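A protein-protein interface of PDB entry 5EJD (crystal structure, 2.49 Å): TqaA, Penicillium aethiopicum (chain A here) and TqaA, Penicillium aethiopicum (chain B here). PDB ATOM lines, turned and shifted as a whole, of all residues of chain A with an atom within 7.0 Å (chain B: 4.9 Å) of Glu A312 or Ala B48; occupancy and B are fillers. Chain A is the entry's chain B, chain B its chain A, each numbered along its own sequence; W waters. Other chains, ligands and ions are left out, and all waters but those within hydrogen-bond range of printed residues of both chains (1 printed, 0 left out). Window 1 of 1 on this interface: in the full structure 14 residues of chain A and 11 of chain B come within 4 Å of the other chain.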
ATOM      1  N   VAL A 175       3.801 -20.799   6.552  1.00  0.00           N
ATOM      2  CA  VAL A 175       3.235 -19.485   6.529  1.00  0.00           C
ATOM      3  C   VAL A 175       1.803 -19.462   7.058  1.00  0.00           C
ATOM      4  O   VAL A 175       1.416 -18.536   7.736  1.00  0.00           O
ATOM      5  CB  VAL A 175       3.229 -18.953   5.107  1.00  0.00           C
ATOM      6  CG1 VAL A 175       2.439 -17.661   5.031  1.00  0.00           C
ATOM      7  CG2 VAL A 175       4.654 -18.754   4.629  1.00  0.00           C
ATOM      8  N   SER A 176       1.025 -20.487   6.756  1.00  0.00           N
ATOM      9  CA  SER A 176      -0.421 -20.453   6.950  1.00  0.00           C
ATOM     10  C   SER A 176      -0.923 -21.245   8.194  1.00  0.00           C
ATOM     11  O   SER A 176      -1.967 -20.937   8.727  1.00  0.00           O
ATOM     12  CB  SER A 176      -1.123 -20.963   5.660  1.00  0.00           C
ATOM     13  OG  SER A 176      -0.944 -22.384   5.473  1.00  0.00           O
ATOM     14  N   LYS A 179      -2.345 -19.306  11.117  1.00  0.00           N
ATOM     15  CA  LYS A 179      -3.657 -18.777  10.872  1.00  0.00           C
ATOM     16  C   LYS A 179      -4.713 -19.768  11.232  1.00  0.00           C
ATOM     17  O   LYS A 179      -5.792 -19.398  11.601  1.00  0.00           O
ATOM     18  CB  LYS A 179      -3.766 -18.339   9.419  1.00  0.00           C
ATOM     19  CG  LYS A 179      -3.203 -16.944   9.276  1.00  0.00           C
ATOM     20  CD  LYS A 179      -4.155 -16.005   8.597  1.00  0.00           C
ATOM     21  CE  LYS A 179      -3.856 -14.557   8.894  1.00  0.00           C
ATOM     22  NZ  LYS A 179      -2.438 -14.275   9.190  1.00  0.00           N
ATOM     23  N   ARG A 304       4.258 -17.997  -2.604  1.00  0.00           N
ATOM     24  CA  ARG A 304       3.224 -17.005  -2.353  1.00  0.00           C
ATOM     25  C   ARG A 304       3.566 -15.619  -2.927  1.00  0.00           C
ATOM     26  O   ARG A 304       2.988 -14.634  -2.518  1.00  0.00           O
ATOM     27  CB  ARG A 304       2.848 -17.007  -0.840  1.00  0.00           C
ATOM     28  CG  ARG A 304       2.037 -18.273  -0.496  1.00  0.00           C
ATOM     29  CD  ARG A 304       2.041 -18.763   0.959  1.00  0.00           C
ATOM     30  NE  ARG A 304       0.720 -18.603   1.476  1.00  0.00           N
ATOM     31  CZ  ARG A 304      -0.099 -19.532   1.922  1.00  0.00           C
ATOM     32  NH1 ARG A 304       0.201 -20.796   2.038  1.00  0.00           N
ATOM     33  NH2 ARG A 304      -1.268 -19.124   2.298  1.00  0.00           N
ATOM     34  N   ASN A 305       4.520 -15.561  -3.871  1.00  0.00           N
ATOM     35  CA  ASN A 305       4.891 -14.314  -4.508  1.00  0.00           C
ATOM     36  C   ASN A 305       4.061 -14.087  -5.771  1.00  0.00           C
ATOM     37  O   ASN A 305       4.591 -13.913  -6.839  1.00  0.00           O
ATOM     38  CB  ASN A 305       6.406 -14.239  -4.816  1.00  0.00           C
ATOM     39  CG  ASN A 305       6.827 -12.870  -5.403  1.00  0.00           C
ATOM     40  OD1 ASN A 305       6.350 -11.778  -4.978  1.00  0.00           O
ATOM     41  ND2 ASN A 305       7.681 -12.914  -6.423  1.00  0.00           N
ATOM     42  N   LEU A 306       2.744 -14.094  -5.618  1.00  0.00           N
ATOM     43  CA  LEU A 306       1.841 -13.970  -6.742  1.00  0.00           C
ATOM     44  C   LEU A 306       0.835 -12.888  -6.428  1.00  0.00           C
ATOM     45  O   LEU A 306       0.466 -12.679  -5.257  1.00  0.00           O
ATOM     46  CB  LEU A 306       1.091 -15.262  -6.974  1.00  0.00           C
ATOM     47  CG  LEU A 306       1.882 -16.430  -7.527  1.00  0.00           C
ATOM     48  CD1 LEU A 306       1.019 -17.683  -7.561  1.00  0.00           C
ATOM     49  CD2 LEU A 306       2.383 -16.121  -8.916  1.00  0.00           C
ATOM     50  N   MET A 308      -2.328 -12.186  -6.016  1.00  0.00           N
ATOM     51  CA  MET A 308      -3.672 -12.674  -5.797  1.00  0.00           C
ATOM     52  C   MET A 308      -4.128 -12.234  -4.426  1.00  0.00           C
ATOM     53  O   MET A 308      -3.340 -12.179  -3.493  1.00  0.00           O
ATOM     54  CB  MET A 308      -3.678 -14.206  -5.899  1.00  0.00           C
ATOM     55  CG  MET A 308      -4.698 -14.887  -5.014  1.00  0.00           C
ATOM     56  SD  MET A 308      -4.728 -16.671  -4.963  1.00  0.00           S
ATOM     57  CE  MET A 308      -3.064 -16.992  -5.480  1.00  0.00           C
ATOM     58  N   ASP A 309      -5.416 -11.968  -4.269  1.00  0.00           N
ATOM     59  CA  ASP A 309      -5.930 -11.504  -2.995  1.00  0.00           C
ATOM     60  C   ASP A 309      -5.782 -12.580  -1.945  1.00  0.00           C
ATOM     61  O   ASP A 309      -6.062 -13.760  -2.210  1.00  0.00           O
ATOM     62  CB  ASP A 309      -7.405 -11.103  -3.117  1.00  0.00           C
ATOM     63  CG  ASP A 309      -7.598  -9.811  -3.935  1.00  0.00           C
ATOM     64  OD1 ASP A 309      -6.604  -9.074  -4.174  1.00  0.00           O
ATOM     65  OD2 ASP A 309      -8.765  -9.506  -4.288  1.00  0.00           O
ATOM     66  N   ASN A 310      -5.347 -12.153  -0.755  1.00  0.00           N
ATOM     67  CA  ASN A 310      -5.204 -13.013   0.414  1.00  0.00           C
ATOM     68  C   ASN A 310      -4.210 -14.123   0.238  1.00  0.00           C
ATOM     69  O   ASN A 310      -4.229 -15.105   0.985  1.00  0.00           O
ATOM     70  CB  ASN A 310      -6.532 -13.678   0.812  1.00  0.00           C
ATOM     71  CG  ASN A 310      -7.631 -12.680   1.093  1.00  0.00           C
ATOM     72  OD1 ASN A 310      -7.406 -11.653   1.721  1.00  0.00           O
ATOM     73  ND2 ASN A 310      -8.827 -13.000   0.642  1.00  0.00           N
ATOM     74  N   ILE A 311      -3.272 -13.957  -0.673  1.00  0.00           N
ATOM     75  CA  ILE A 311      -2.309 -15.015  -0.850  1.00  0.00           C
ATOM     76  C   ILE A 311      -1.425 -15.245   0.365  1.00  0.00           C
ATOM     77  O   ILE A 311      -0.897 -16.343   0.552  1.00  0.00           O
ATOM     78  CB  ILE A 311      -1.441 -14.823  -2.105  1.00  0.00           C
ATOM     79  CG1 ILE A 311      -0.832 -16.174  -2.441  1.00  0.00           C
ATOM     80  CG2 ILE A 311      -0.455 -13.697  -1.913  1.00  0.00           C
ATOM     81  CD1 ILE A 311      -0.092 -16.167  -3.708  1.00  0.00           C
ATOM     82  N   GLU A 312      -1.261 -14.227   1.204  1.00  0.00           N
ATOM     83  CA  GLU A 312      -0.412 -14.340   2.405  1.00  0.00           C
ATOM     84  C   GLU A 312      -1.078 -15.114   3.545  1.00  0.00           C
ATOM     85  O   GLU A 312      -0.388 -15.575   4.432  1.00  0.00           O
ATOM     86  CB  GLU A 312       0.004 -12.955   2.923  1.00  0.00           C
ATOM     87  CG  GLU A 312      -1.033 -12.231   3.776  1.00  0.00           C
ATOM     88  CD  GLU A 312      -2.182 -11.565   2.996  1.00  0.00           C
ATOM     89  OE1 GLU A 312      -2.336 -11.757   1.740  1.00  0.00           O
ATOM     90  OE2 GLU A 312      -2.942 -10.823   3.668  1.00  0.00           O
ATOM     91  N   SER A 313      -2.395 -15.250   3.513  1.00  0.00           N
ATOM     92  CA  SER A 313      -3.108 -15.819   4.626  1.00  0.00           C
ATOM     93  C   SER A 313      -3.896 -17.111   4.323  1.00  0.00           C
ATOM     94  O   SER A 313      -4.333 -17.796   5.254  1.00  0.00           O
ATOM     95  CB  SER A 313      -4.043 -14.754   5.175  1.00  0.00           C
ATOM     96  OG  SER A 313      -5.079 -14.480   4.282  1.00  0.00           O
ATOM     97  N   LEU A 314      -4.074 -17.461   3.061  1.00  0.00           N
ATOM     98  CA  LEU A 314      -4.932 -18.583   2.748  1.00  0.00           C
ATOM     99  C   LEU A 314      -4.361 -19.881   3.259  1.00  0.00           C
ATOM    100  O   LEU A 314      -3.174 -20.079   3.232  1.00  0.00           O
ATOM    101  CB  LEU A 314      -5.242 -18.665   1.269  1.00  0.00           C
ATOM    102  CG  LEU A 314      -4.147 -18.988   0.254  1.00  0.00           C
ATOM    103  CD1 LEU A 314      -3.910 -20.463   0.084  1.00  0.00           C
ATOM    104  CD2 LEU A 314      -4.584 -18.395  -1.087  1.00  0.00           C
ATOM    105  N   MET B  44       7.349 -11.120   1.299  1.00  0.00           N
ATOM    106  CA  MET B  44       6.153 -11.693   0.669  1.00  0.00           C
ATOM    107  C   MET B  44       4.877 -11.061   1.254  1.00  0.00           C
ATOM    108  O   MET B  44       4.022 -10.620   0.498  1.00  0.00           O
ATOM    109  CB  MET B  44       6.166 -13.225   0.764  1.00  0.00           C
ATOM    110  CG  MET B  44       5.224 -14.021   1.662  1.00  0.00           C
ATOM    111  SD  MET B  44       3.687 -14.153   0.965  1.00  0.00           S
ATOM    112  CE  MET B  44       2.641 -13.496   2.115  1.00  0.00           C
ATOM    113  N   LYS B  45       4.790 -10.944   2.573  1.00  0.00           N
ATOM    114  CA  LYS B  45       3.626 -10.310   3.191  1.00  0.00           C
ATOM    115  C   LYS B  45       3.488  -8.826   2.854  1.00  0.00           C
ATOM    116  O   LYS B  45       2.394  -8.357   2.572  1.00  0.00           O
ATOM    117  CB  LYS B  45       3.638 -10.481   4.690  1.00  0.00           C
ATOM    118  CG  LYS B  45       3.703 -11.933   5.087  1.00  0.00           C
ATOM    119  CD  LYS B  45       3.262 -12.183   6.519  1.00  0.00           C
ATOM    120  CE  LYS B  45       4.382 -12.784   7.345  1.00  0.00           C
ATOM    121  NZ  LYS B  45       3.870 -13.857   8.234  1.00  0.00           N
ATOM    122  N   ALA B  46       4.607  -8.135   2.785  1.00  0.00           N
ATOM    123  CA  ALA B  46       4.612  -6.723   2.442  1.00  0.00           C
ATOM    124  C   ALA B  46       4.067  -6.542   1.039  1.00  0.00           C
ATOM    125  O   ALA B  46       3.239  -5.692   0.789  1.00  0.00           O
ATOM    126  CB  ALA B  46       6.009  -6.134   2.536  1.00  0.00           C
ATOM    127  N   SER B  47       4.561  -7.349   0.126  1.00  0.00           N
ATOM    128  CA  SER B  47       4.083  -7.324  -1.234  1.00  0.00           C
ATOM    129  C   SER B  47       2.572  -7.556  -1.335  1.00  0.00           C
ATOM    130  O   SER B  47       1.889  -6.897  -2.110  1.00  0.00           O
ATOM    131  CB  SER B  47       4.842  -8.346  -2.048  1.00  0.00           C
ATOM    132  OG  SER B  47       4.220  -8.465  -3.296  1.00  0.00           O
ATOM    133  N   ALA B  48       2.044  -8.516  -0.576  1.00  0.00           N
ATOM    134  CA  ALA B  48       0.608  -8.776  -0.596  1.00  0.00           C
ATOM    135  C   ALA B  48      -0.207  -7.608  -0.009  1.00  0.00           C
ATOM    136  O   ALA B  48      -1.251  -7.280  -0.517  1.00  0.00           O
ATOM    137  CB  ALA B  48       0.290 -10.047   0.148  1.00  0.00           C
ATOM    138  N   LEU B  49       0.265  -7.024   1.075  1.00  0.00           N
ATOM    139  CA  LEU B  49      -0.393  -5.872   1.645  1.00  0.00           C
ATOM    140  C   LEU B  49      -0.307  -4.669   0.711  1.00  0.00           C
ATOM    141  O   LEU B  49      -1.235  -3.876   0.644  1.00  0.00           O
ATOM    142  CB  LEU B  49       0.219  -5.536   3.002  1.00  0.00           C
ATOM    143  CG  LEU B  49      -0.592  -5.939   4.241  1.00  0.00           C
ATOM    144  CD1 LEU B  49      -1.193  -7.326   4.184  1.00  0.00           C
ATOM    145  CD2 LEU B  49       0.320  -5.844   5.449  1.00  0.00           C
ATOM    146  N   GLY B  50       0.802  -4.559  -0.020  1.00  0.00           N
ATOM    147  CA  GLY B  50       0.945  -3.583  -1.091  1.00  0.00           C
ATOM    148  C   GLY B  50      -0.214  -3.665  -2.078  1.00  0.00           C
ATOM    149  O   GLY B  50      -0.857  -2.689  -2.387  1.00  0.00           O
ATOM    150  N   ARG B  51      -0.467  -4.853  -2.591  1.00  0.00           N
ATOM    151  CA  ARG B  51      -1.545  -5.037  -3.522  1.00  0.00           C
ATOM    152  C   ARG B  51      -2.876  -4.606  -2.950  1.00  0.00           C
ATOM    153  O   ARG B  51      -3.617  -3.960  -3.621  1.00  0.00           O
ATOM    154  CB  ARG B  51      -1.612  -6.477  -3.925  1.00  0.00           C
ATOM    155  CG  ARG B  51      -2.751  -6.808  -4.844  1.00  0.00           C
ATOM    156  CD  ARG B  51      -2.782  -8.290  -5.203  1.00  0.00           C
ATOM    157  NE  ARG B  51      -3.976  -8.606  -5.955  1.00  0.00           N
ATOM    158  CZ  ARG B  51      -4.088  -8.362  -7.257  1.00  0.00           C
ATOM    159  NH1 ARG B  51      -5.212  -8.675  -7.882  1.00  0.00           N
ATOM    160  NH2 ARG B  51      -3.082  -7.794  -7.935  1.00  0.00           N
ATOM    161  N   ALA B  52      -3.188  -4.971  -1.728  1.00  0.00           N
ATOM    162  CA  ALA B  52      -4.457  -4.578  -1.122  1.00  0.00           C
ATOM    163  C   ALA B  52      -4.585  -3.068  -0.939  1.00  0.00           C
ATOM    164  O   ALA B  52      -5.683  -2.551  -0.861  1.00  0.00           O
ATOM    165  CB  ALA B  52      -4.652  -5.278   0.222  1.00  0.00           C
HETATM  166  O   HOH W   1       2.790 -11.927  -1.880  1.00  0.00           O
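Water W1 lies within hydrogen-bond range of O of Arg A304 (2.8 Å) and O of Met B44 (3.0 Å).
Hydrophobic or aromatic side chains of chain B within 4 Å of the printed part of chain A: Met B44, Ala B48 and Leu B49. Along chain A the printed residues that touch a printed residue of chain B span positions 304 to 312. Among the printed residues, Asp or Glu carboxylates within 4 Å of a Lys or Arg side-chain nitrogen of the other chain: Asp A309 with Arg B51 (3.2 Å).
Printed residues of chain B within 4 Å of Met A308: Arg B51. Printed residues of chain B within 4 Å of Asp A309: Arg B51. Of chain B, only Met B44 (2.8 Å), Ala B48 (3.5 Å) and Leu B49 (3.9 Å) come within 4 Å of Glu A312. Of the printed residues of chain A, Met B44 touches Arg A304 (3.5 Å) and Glu A312 (2.8 Å). Of chain A, only Glu A312 comes within 4 Å of Ala B48. Of the printed residues of chain A, Arg B51 touches Met A308 and Asp A309. The nearest residue of chain B that does not touch Glu A312 is Lys B45 (4.4 Å). The nearest residue of chain A that does not touch Ala B48 is Ile A311 (4.3 Å).
Arg B51 touches Met A308 (NE to C, 3.9 Å). Met B44 touches Glu A312 (CE to CB, 2.8 Å). Glu A312 touches Ala B48 (OE1 to CB, 3.5 Å). Glu A312 touches Leu B49.
The guanidinium group of Arg A304 lies within hydrogen-bond range of the backbone carbonyl oxygen of Ile A311, 2.9 Å away.
OD1 of Asp A309 lies within salt-bridge range of NE of Arg B51. The side-chain sulfur (SD) of Met B44 lies close to the backbone carbonyl oxygen (O) of Arg A304, at 3.6 Å.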
